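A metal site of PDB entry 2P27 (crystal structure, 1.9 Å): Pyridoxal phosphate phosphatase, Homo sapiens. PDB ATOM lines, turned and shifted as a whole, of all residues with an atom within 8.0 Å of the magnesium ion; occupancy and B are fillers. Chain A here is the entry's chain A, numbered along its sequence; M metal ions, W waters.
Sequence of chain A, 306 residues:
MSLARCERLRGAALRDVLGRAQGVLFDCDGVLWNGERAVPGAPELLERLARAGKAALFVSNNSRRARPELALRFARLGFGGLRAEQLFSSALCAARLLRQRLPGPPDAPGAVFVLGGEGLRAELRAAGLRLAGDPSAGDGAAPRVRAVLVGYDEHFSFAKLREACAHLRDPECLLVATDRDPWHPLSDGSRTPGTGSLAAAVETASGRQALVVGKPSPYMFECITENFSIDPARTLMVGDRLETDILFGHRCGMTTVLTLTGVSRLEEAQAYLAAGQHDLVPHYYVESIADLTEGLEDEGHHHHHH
The magnesium ion is bound by OD2 of Asp 27 (2.0 Å), OD1 of Asp 240 (2.0 Å), water W1 (2.1 Å), O of Asp 29 (2.1 Å), water W3 (2.1 Å) and water W2 (2.2 Å). The magnesium ion has six donor atoms within binding distance.
Water W3 lies within hydrogen-bond range of the side-chain carboxylate (OD2) of Asp 245 (2.7 Å) and the side-chain carboxylate (OD1) of Asp 27 (3.5 Å).
The side-chain carboxylate of Asp 245 sits at hydrogen-bond distance from the backbone NH of Arg 241 (3.0 Å). The backbone NH of Ser 264 sits at hydrogen-bond distance from the backbone carbonyl oxygen of Asp 240, at 2.8 Å. The side-chain amino group (NZ) of Lys 215 is in salt-bridge range of the side-chain carboxylate (OD1) of Asp 245. N of Val 263 sits at hydrogen-bond distance from OD2 of Asp 240, 2.8 Å away. OD2 of Asp 245 is in hydrogen-bond range of N of Asp 240 (3.1 Å). NZ of Lys 215 lies within salt-bridge range of OD1 of Asp 27. The backbone carbonyl oxygen (O) of Val 238 sits at hydrogen-bond distance from the backbone NH (N) of Asp 27 (2.9 Å).
Merely in contact with the magnesium ion: Asp 245 (3.97 Å).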
ATOM      1  N   PHE A  26     -10.869  13.778   9.750  1.00  0.00           N
ATOM      2  CA  PHE A  26     -11.210  14.922  10.571  1.00  0.00           C
ATOM      3  C   PHE A  26     -10.023  15.353  11.437  1.00  0.00           C
ATOM      4  O   PHE A  26      -9.409  14.529  12.133  1.00  0.00           O
ATOM      5  CB  PHE A  26     -12.308  14.531  11.558  1.00  0.00           C
ATOM      6  CG  PHE A  26     -13.670  14.324  10.928  1.00  0.00           C
ATOM      7  CD1 PHE A  26     -14.500  15.399  10.650  1.00  0.00           C
ATOM      8  CD2 PHE A  26     -14.113  13.030  10.650  1.00  0.00           C
ATOM      9  CE1 PHE A  26     -15.781  15.205  10.094  1.00  0.00           C
ATOM     10  CE2 PHE A  26     -15.391  12.815  10.103  1.00  0.00           C
ATOM     11  CZ  PHE A  26     -16.223  13.907   9.830  1.00  0.00           C
ATOM     12  N   ASP A  27      -9.733  16.657  11.436  1.00  0.00           N
ATOM     13  CA  ASP A  27      -9.028  17.267  12.564  1.00  0.00           C
ATOM     14  C   ASP A  27      -9.981  17.251  13.795  1.00  0.00           C
ATOM     15  O   ASP A  27     -11.198  17.101  13.627  1.00  0.00           O
ATOM     16  CB  ASP A  27      -8.615  18.691  12.204  1.00  0.00           C
ATOM     17  CG  ASP A  27      -8.082  19.457  13.367  1.00  0.00           C
ATOM     18  OD1 ASP A  27      -7.137  18.984  14.041  1.00  0.00           O
ATOM     19  OD2 ASP A  27      -8.640  20.528  13.621  1.00  0.00           O
ATOM     20  N   CYS A  28      -9.448  17.353  15.010  1.00  0.00           N
ATOM     21  CA  CYS A  28     -10.335  17.283  16.189  1.00  0.00           C
ATOM     22  C   CYS A  28     -10.667  18.651  16.811  1.00  0.00           C
ATOM     23  O   CYS A  28     -11.827  19.081  16.803  1.00  0.00           O
ATOM     24  CB  CYS A  28      -9.768  16.310  17.250  1.00  0.00           C
ATOM     25  SG  CYS A  28      -9.400  14.667  16.522  1.00  0.00           S
ATOM     26  N   ASP A  29      -9.655  19.337  17.344  1.00  0.00           N
ATOM     27  CA  ASP A  29      -9.902  20.580  18.064  1.00  0.00           C
ATOM     28  C   ASP A  29     -10.301  21.695  17.093  1.00  0.00           C
ATOM     29  O   ASP A  29      -9.647  21.915  16.089  1.00  0.00           O
ATOM     30  CB  ASP A  29      -8.684  20.980  18.900  1.00  0.00           C
ATOM     31  CG  ASP A  29      -9.033  21.898  20.065  1.00  0.00           C
ATOM     32  OD1 ASP A  29     -10.214  21.975  20.472  1.00  0.00           O
ATOM     33  OD2 ASP A  29      -8.107  22.545  20.606  1.00  0.00           O
ATOM     34  N   GLY A  30     -11.396  22.389  17.404  1.00  0.00           N
ATOM     35  CA  GLY A  30     -11.963  23.376  16.507  1.00  0.00           C
ATOM     36  C   GLY A  30     -12.903  22.776  15.468  1.00  0.00           C
ATOM     37  O   GLY A  30     -13.427  23.502  14.643  1.00  0.00           O
ATOM     38  N   VAL A  31     -13.122  21.459  15.500  1.00  0.00           N
ATOM     39  CA  VAL A  31     -13.885  20.753  14.467  1.00  0.00           C
ATOM     40  C   VAL A  31     -14.968  19.896  15.103  1.00  0.00           C
ATOM     41  O   VAL A  31     -16.167  20.106  14.865  1.00  0.00           O
ATOM     42  CB  VAL A  31     -12.955  19.864  13.571  1.00  0.00           C
ATOM     43  CG1 VAL A  31     -13.773  18.987  12.606  1.00  0.00           C
ATOM     44  CG2 VAL A  31     -11.947  20.736  12.780  1.00  0.00           C
ATOM     45  N   LEU A  32     -14.543  18.941  15.925  1.00  0.00           N
ATOM     46  CA  LEU A  32     -15.455  18.088  16.674  1.00  0.00           C
ATOM     47  C   LEU A  32     -15.885  18.723  17.989  1.00  0.00           C
ATOM     48  O   LEU A  32     -16.978  18.441  18.522  1.00  0.00           O
ATOM     49  CB  LEU A  32     -14.777  16.750  16.970  1.00  0.00           C
ATOM     50  CG  LEU A  32     -14.209  15.945  15.812  1.00  0.00           C
ATOM     51  CD1 LEU A  32     -13.456  14.694  16.376  1.00  0.00           C
ATOM     52  CD2 LEU A  32     -15.319  15.567  14.855  1.00  0.00           C
ATOM     53  N   TRP A  33     -15.013  19.559  18.542  1.00  0.00           N
ATOM     54  CA  TRP A  33     -15.225  20.185  19.843  1.00  0.00           C
ATOM     55  C   TRP A  33     -14.347  21.415  19.954  1.00  0.00           C
ATOM     56  O   TRP A  33     -13.450  21.618  19.122  1.00  0.00           O
ATOM     57  CB  TRP A  33     -14.898  19.187  20.969  1.00  0.00           C
ATOM     58  CG  TRP A  33     -13.550  18.511  20.831  1.00  0.00           C
ATOM     59  CD1 TRP A  33     -12.334  19.103  20.956  1.00  0.00           C
ATOM     60  CD2 TRP A  33     -13.304  17.115  20.598  1.00  0.00           C
ATOM     61  NE1 TRP A  33     -11.328  18.165  20.797  1.00  0.00           N
ATOM     62  CE2 TRP A  33     -11.899  16.934  20.582  1.00  0.00           C
ATOM     63  CE3 TRP A  33     -14.125  15.987  20.437  1.00  0.00           C
ATOM     64  CZ2 TRP A  33     -11.287  15.669  20.402  1.00  0.00           C
ATOM     65  CZ3 TRP A  33     -13.519  14.739  20.210  1.00  0.00           C
ATOM     66  CH2 TRP A  33     -12.117  14.591  20.203  1.00  0.00           C
ATOM     67  N   ASN A  34     -14.634  22.264  20.941  1.00  0.00           N
ATOM     68  CA  ASN A  34     -13.721  23.296  21.396  1.00  0.00           C
ATOM     69  C   ASN A  34     -13.586  23.086  22.908  1.00  0.00           C
ATOM     70  O   ASN A  34     -14.574  23.268  23.649  1.00  0.00           O
ATOM     71  CB  ASN A  34     -14.267  24.691  21.133  1.00  0.00           C
ATOM     72  CG  ASN A  34     -14.386  25.000  19.660  1.00  0.00           C
ATOM     73  OD1 ASN A  34     -15.490  25.003  19.113  1.00  0.00           O
ATOM     74  ND2 ASN A  34     -13.260  25.221  19.002  1.00  0.00           N
ATOM     75  N   VAL A  59      -7.108  12.897  12.577  1.00  0.00           N
ATOM     76  CA  VAL A  59      -5.720  13.288  12.370  1.00  0.00           C
ATOM     77  C   VAL A  59      -5.441  14.514  13.218  1.00  0.00           C
ATOM     78  O   VAL A  59      -5.952  15.583  12.931  1.00  0.00           O
ATOM     79  CB  VAL A  59      -5.432  13.631  10.881  1.00  0.00           C
ATOM     80  CG1 VAL A  59      -3.954  13.927  10.677  1.00  0.00           C
ATOM     81  CG2 VAL A  59      -5.870  12.491   9.949  1.00  0.00           C
ATOM     82  N   SER A  60      -4.622  14.368  14.255  1.00  0.00           N
ATOM     83  CA  SER A  60      -4.395  15.438  15.225  1.00  0.00           C
ATOM     84  C   SER A  60      -2.908  15.742  15.373  1.00  0.00           C
ATOM     85  O   SER A  60      -2.099  14.819  15.442  1.00  0.00           O
ATOM     86  CB  SER A  60      -4.939  15.007  16.582  1.00  0.00           C
ATOM     87  OG  SER A  60      -4.670  15.974  17.569  1.00  0.00           O
ATOM     88  N   ASN A  61      -2.546  17.018  15.459  1.00  0.00           N
ATOM     89  CA  ASN A  61      -1.167  17.386  15.837  1.00  0.00           C
ATOM     90  C   ASN A  61      -0.821  17.242  17.324  1.00  0.00           C
ATOM     91  O   ASN A  61       0.297  17.552  17.746  1.00  0.00           O
ATOM     92  CB  ASN A  61      -0.823  18.804  15.310  1.00  0.00           C
ATOM     93  CG  ASN A  61      -0.463  18.785  13.830  1.00  0.00           C
ATOM     94  OD1 ASN A  61      -0.287  17.715  13.229  1.00  0.00           O
ATOM     95  ND2 ASN A  61      -0.350  19.975  13.229  1.00  0.00           N
ATOM     96  N   ASP A 181       2.616  23.969  14.756  1.00  0.00           N
ATOM     97  CA  ASP A 181       1.516  24.860  15.139  1.00  0.00           C
ATOM     98  C   ASP A 181       2.085  25.917  16.090  1.00  0.00           C
ATOM     99  O   ASP A 181       2.749  25.573  17.081  1.00  0.00           O
ATOM    100  CB  ASP A 181       0.389  24.082  15.803  1.00  0.00           C
ATOM    101  CG  ASP A 181      -0.302  23.113  14.848  1.00  0.00           C
ATOM    102  OD1 ASP A 181      -0.151  23.217  13.616  1.00  0.00           O
ATOM    103  OD2 ASP A 181      -1.025  22.258  15.359  1.00  0.00           O
ATOM    104  N   HIS A 184      -2.119  27.769  20.272  1.00  0.00           N
ATOM    105  CA  HIS A 184      -3.432  27.124  20.347  1.00  0.00           C
ATOM    106  C   HIS A 184      -4.356  27.947  21.226  1.00  0.00           C
ATOM    107  O   HIS A 184      -3.924  28.449  22.268  1.00  0.00           O
ATOM    108  CB  HIS A 184      -3.293  25.715  20.909  1.00  0.00           C
ATOM    109  CG  HIS A 184      -2.437  24.826  20.058  1.00  0.00           C
ATOM    110  ND1 HIS A 184      -2.866  24.329  18.836  1.00  0.00           N
ATOM    111  CD2 HIS A 184      -1.163  24.400  20.211  1.00  0.00           C
ATOM    112  CE1 HIS A 184      -1.905  23.609  18.295  1.00  0.00           C
ATOM    113  NE2 HIS A 184      -0.859  23.637  19.100  1.00  0.00           N
ATOM    114  N   PRO A 185      -5.636  28.088  20.806  1.00  0.00           N
ATOM    115  CA  PRO A 185      -6.590  28.829  21.643  1.00  0.00           C
ATOM    116  C   PRO A 185      -7.106  27.976  22.806  1.00  0.00           C
ATOM    117  O   PRO A 185      -7.222  26.741  22.688  1.00  0.00           O
ATOM    118  CB  PRO A 185      -7.724  29.167  20.685  1.00  0.00           C
ATOM    119  CG  PRO A 185      -7.708  28.068  19.650  1.00  0.00           C
ATOM    120  CD  PRO A 185      -6.262  27.598  19.561  1.00  0.00           C
ATOM    121  N   LYS A 215       0.702  17.440  10.450  1.00  0.00           N
ATOM    122  CA  LYS A 215       0.181  18.304   9.412  1.00  0.00           C
ATOM    123  C   LYS A 215       0.868  19.667   9.547  1.00  0.00           C
ATOM    124  O   LYS A 215       1.113  20.107  10.673  1.00  0.00           O
ATOM    125  CB  LYS A 215      -1.329  18.530   9.594  1.00  0.00           C
ATOM    126  CG  LYS A 215      -2.191  17.274   9.877  1.00  0.00           C
ATOM    127  CD  LYS A 215      -3.591  17.699  10.347  1.00  0.00           C
ATOM    128  CE  LYS A 215      -3.591  17.956  11.856  1.00  0.00           C
ATOM    129  NZ  LYS A 215      -4.961  18.330  12.327  1.00  0.00           N
ATOM    130  N   MET A 237     -10.975  16.027   3.601  1.00  0.00           N
ATOM    131  CA  MET A 237     -10.158  16.485   4.731  1.00  0.00           C
ATOM    132  C   MET A 237     -10.832  17.690   5.386  1.00  0.00           C
ATOM    133  O   MET A 237     -11.007  18.741   4.765  1.00  0.00           O
ATOM    134  CB  MET A 237      -8.721  16.822   4.283  1.00  0.00           C
ATOM    135  CG  MET A 237      -7.814  17.420   5.366  1.00  0.00           C
ATOM    136  SD  MET A 237      -7.552  16.201   6.913  1.00  0.00           S
ATOM    137  CE  MET A 237      -7.307  17.568   8.322  1.00  0.00           C
ATOM    138  N   VAL A 238     -11.223  17.522   6.652  1.00  0.00           N
ATOM    139  CA  VAL A 238     -12.019  18.519   7.331  1.00  0.00           C
ATOM    140  C   VAL A 238     -11.241  19.149   8.476  1.00  0.00           C
ATOM    141  O   VAL A 238     -10.800  18.440   9.395  1.00  0.00           O
ATOM    142  CB  VAL A 238     -13.367  17.927   7.873  1.00  0.00           C
ATOM    143  CG1 VAL A 238     -14.169  18.994   8.555  1.00  0.00           C
ATOM    144  CG2 VAL A 238     -14.199  17.299   6.722  1.00  0.00           C
ATOM    145  N   GLY A 239     -11.076  20.470   8.439  1.00  0.00           N
ATOM    146  CA  GLY A 239     -10.252  21.135   9.461  1.00  0.00           C
ATOM    147  C   GLY A 239     -10.634  22.579   9.651  1.00  0.00           C
ATOM    148  O   GLY A 239     -11.401  23.130   8.868  1.00  0.00           O
ATOM    149  N   ASP A 240     -10.120  23.183  10.716  1.00  0.00           N
ATOM    150  CA  ASP A 240     -10.399  24.583  11.038  1.00  0.00           C
ATOM    151  C   ASP A 240      -9.212  25.492  10.821  1.00  0.00           C
ATOM    152  O   ASP A 240      -9.353  26.720  10.951  1.00  0.00           O
ATOM    153  CB  ASP A 240     -10.852  24.720  12.492  1.00  0.00           C
ATOM    154  CG  ASP A 240      -9.730  24.393  13.475  1.00  0.00           C
ATOM    155  OD1 ASP A 240      -9.257  23.228  13.469  1.00  0.00           O
ATOM    156  OD2 ASP A 240      -9.323  25.272  14.247  1.00  0.00           O
ATOM    157  N   ARG A 241      -8.045  24.921  10.495  1.00  0.00           N
ATOM    158  CA  ARG A 241      -6.823  25.717  10.380  1.00  0.00           C
ATOM    159  C   ARG A 241      -6.243  25.624   8.963  1.00  0.00           C
ATOM    160  O   ARG A 241      -5.833  24.551   8.523  1.00  0.00           O
ATOM    161  CB  ARG A 241      -5.796  25.251  11.433  1.00  0.00           C
ATOM    162  CG  ARG A 241      -4.787  26.308  11.819  1.00  0.00           C
ATOM    163  CD  ARG A 241      -4.161  25.997  13.161  1.00  0.00           C
ATOM    164  NE  ARG A 241      -3.406  27.147  13.665  1.00  0.00           N
ATOM    165  CZ  ARG A 241      -3.003  27.335  14.920  1.00  0.00           C
ATOM    166  NH1 ARG A 241      -2.340  28.447  15.233  1.00  0.00           N
ATOM    167  NH2 ARG A 241      -3.254  26.427  15.872  1.00  0.00           N
ATOM    168  N   THR A 244      -2.529  24.487   8.372  1.00  0.00           N
ATOM    169  CA  THR A 244      -2.258  23.161   8.907  1.00  0.00           C
ATOM    170  C   THR A 244      -3.123  22.092   8.216  1.00  0.00           C
ATOM    171  O   THR A 244      -2.591  21.211   7.529  1.00  0.00           O
ATOM    172  CB  THR A 244      -2.493  23.156  10.451  1.00  0.00           C
ATOM    173  OG1 THR A 244      -1.508  24.017  11.065  1.00  0.00           O
ATOM    174  CG2 THR A 244      -2.322  21.752  11.027  1.00  0.00           C
ATOM    175  N   ASP A 245      -4.438  22.191   8.398  1.00  0.00           N
ATOM    176  CA  ASP A 245      -5.378  21.187   7.892  1.00  0.00           C
ATOM    177  C   ASP A 245      -5.620  21.270   6.402  1.00  0.00           C
ATOM    178  O   ASP A 245      -5.628  20.237   5.712  1.00  0.00           O
ATOM    179  CB  ASP A 245      -6.727  21.318   8.623  1.00  0.00           C
ATOM    180  CG  ASP A 245      -6.587  21.231  10.122  1.00  0.00           C
ATOM    181  OD1 ASP A 245      -5.844  20.329  10.605  1.00  0.00           O
ATOM    182  OD2 ASP A 245      -7.193  22.072  10.822  1.00  0.00           O
ATOM    183  N   THR A 259     -14.054  24.184   8.303  1.00  0.00           N
ATOM    184  CA  THR A 259     -15.140  24.463   9.217  1.00  0.00           C
ATOM    185  C   THR A 259     -14.811  25.723   9.992  1.00  0.00           C
ATOM    186  O   THR A 259     -13.637  25.995  10.279  1.00  0.00           O
ATOM    187  CB  THR A 259     -15.441  23.281  10.175  1.00  0.00           C
ATOM    188  OG1 THR A 259     -16.612  23.593  10.910  1.00  0.00           O
ATOM    189  CG2 THR A 259     -14.292  23.066  11.149  1.00  0.00           C
ATOM    190  N   THR A 261     -15.810  26.749  13.039  1.00  0.00           N
ATOM    191  CA  THR A 261     -15.894  26.643  14.488  1.00  0.00           C
ATOM    192  C   THR A 261     -14.516  26.705  15.176  1.00  0.00           C
ATOM    193  O   THR A 261     -14.423  26.486  16.381  1.00  0.00           O
ATOM    194  CB  THR A 261     -16.594  25.318  14.909  1.00  0.00           C
ATOM    195  OG1 THR A 261     -16.018  24.215  14.195  1.00  0.00           O
ATOM    196  CG2 THR A 261     -18.115  25.370  14.640  1.00  0.00           C
ATOM    197  N   GLY A 262     -13.456  27.023  14.442  1.00  0.00           N
ATOM    198  CA  GLY A 262     -12.109  26.971  15.029  1.00  0.00           C
ATOM    199  C   GLY A 262     -11.249  28.197  14.747  1.00  0.00           C
ATOM    200  O   GLY A 262     -11.723  29.339  14.798  1.00  0.00           O
ATOM    201  N   VAL A 263      -9.987  27.951  14.441  1.00  0.00           N
ATOM    202  CA  VAL A 263      -8.971  28.995  14.343  1.00  0.00           C
ATOM    203  C   VAL A 263      -9.105  29.934  13.138  1.00  0.00           C
ATOM    204  O   VAL A 263      -9.075  31.170  13.295  1.00  0.00           O
ATOM    205  CB  VAL A 263      -7.555  28.355  14.394  1.00  0.00           C
ATOM    206  CG1 VAL A 263      -6.455  29.366  14.051  1.00  0.00           C
ATOM    207  CG2 VAL A 263      -7.311  27.723  15.768  1.00  0.00           C
ATOM    208  N   SER A 264      -9.245  29.365  11.941  1.00  0.00           N
ATOM    209  CA  SER A 264      -9.193  30.192  10.725  1.00  0.00           C
ATOM    210  C   SER A 264     -10.553  30.794  10.393  1.00  0.00           C
ATOM    211  O   SER A 264     -11.611  30.188  10.683  1.00  0.00           O
ATOM    212  CB  SER A 264      -8.674  29.392   9.527  1.00  0.00           C
ATOM    213  OG  SER A 264      -7.322  28.968   9.743  1.00  0.00           O
HETATM  214 MG    MG M   1      -8.085  22.085  14.692  1.00  0.00          MG
HETATM  215  O   HOH W   1      -6.763  21.005  15.882  1.00  0.00           O
HETATM  216  O   HOH W   2      -7.576  23.978  15.716  1.00  0.00           O
HETATM  217  O   HOH W   3      -6.412  22.345  13.424  1.00  0.00           O
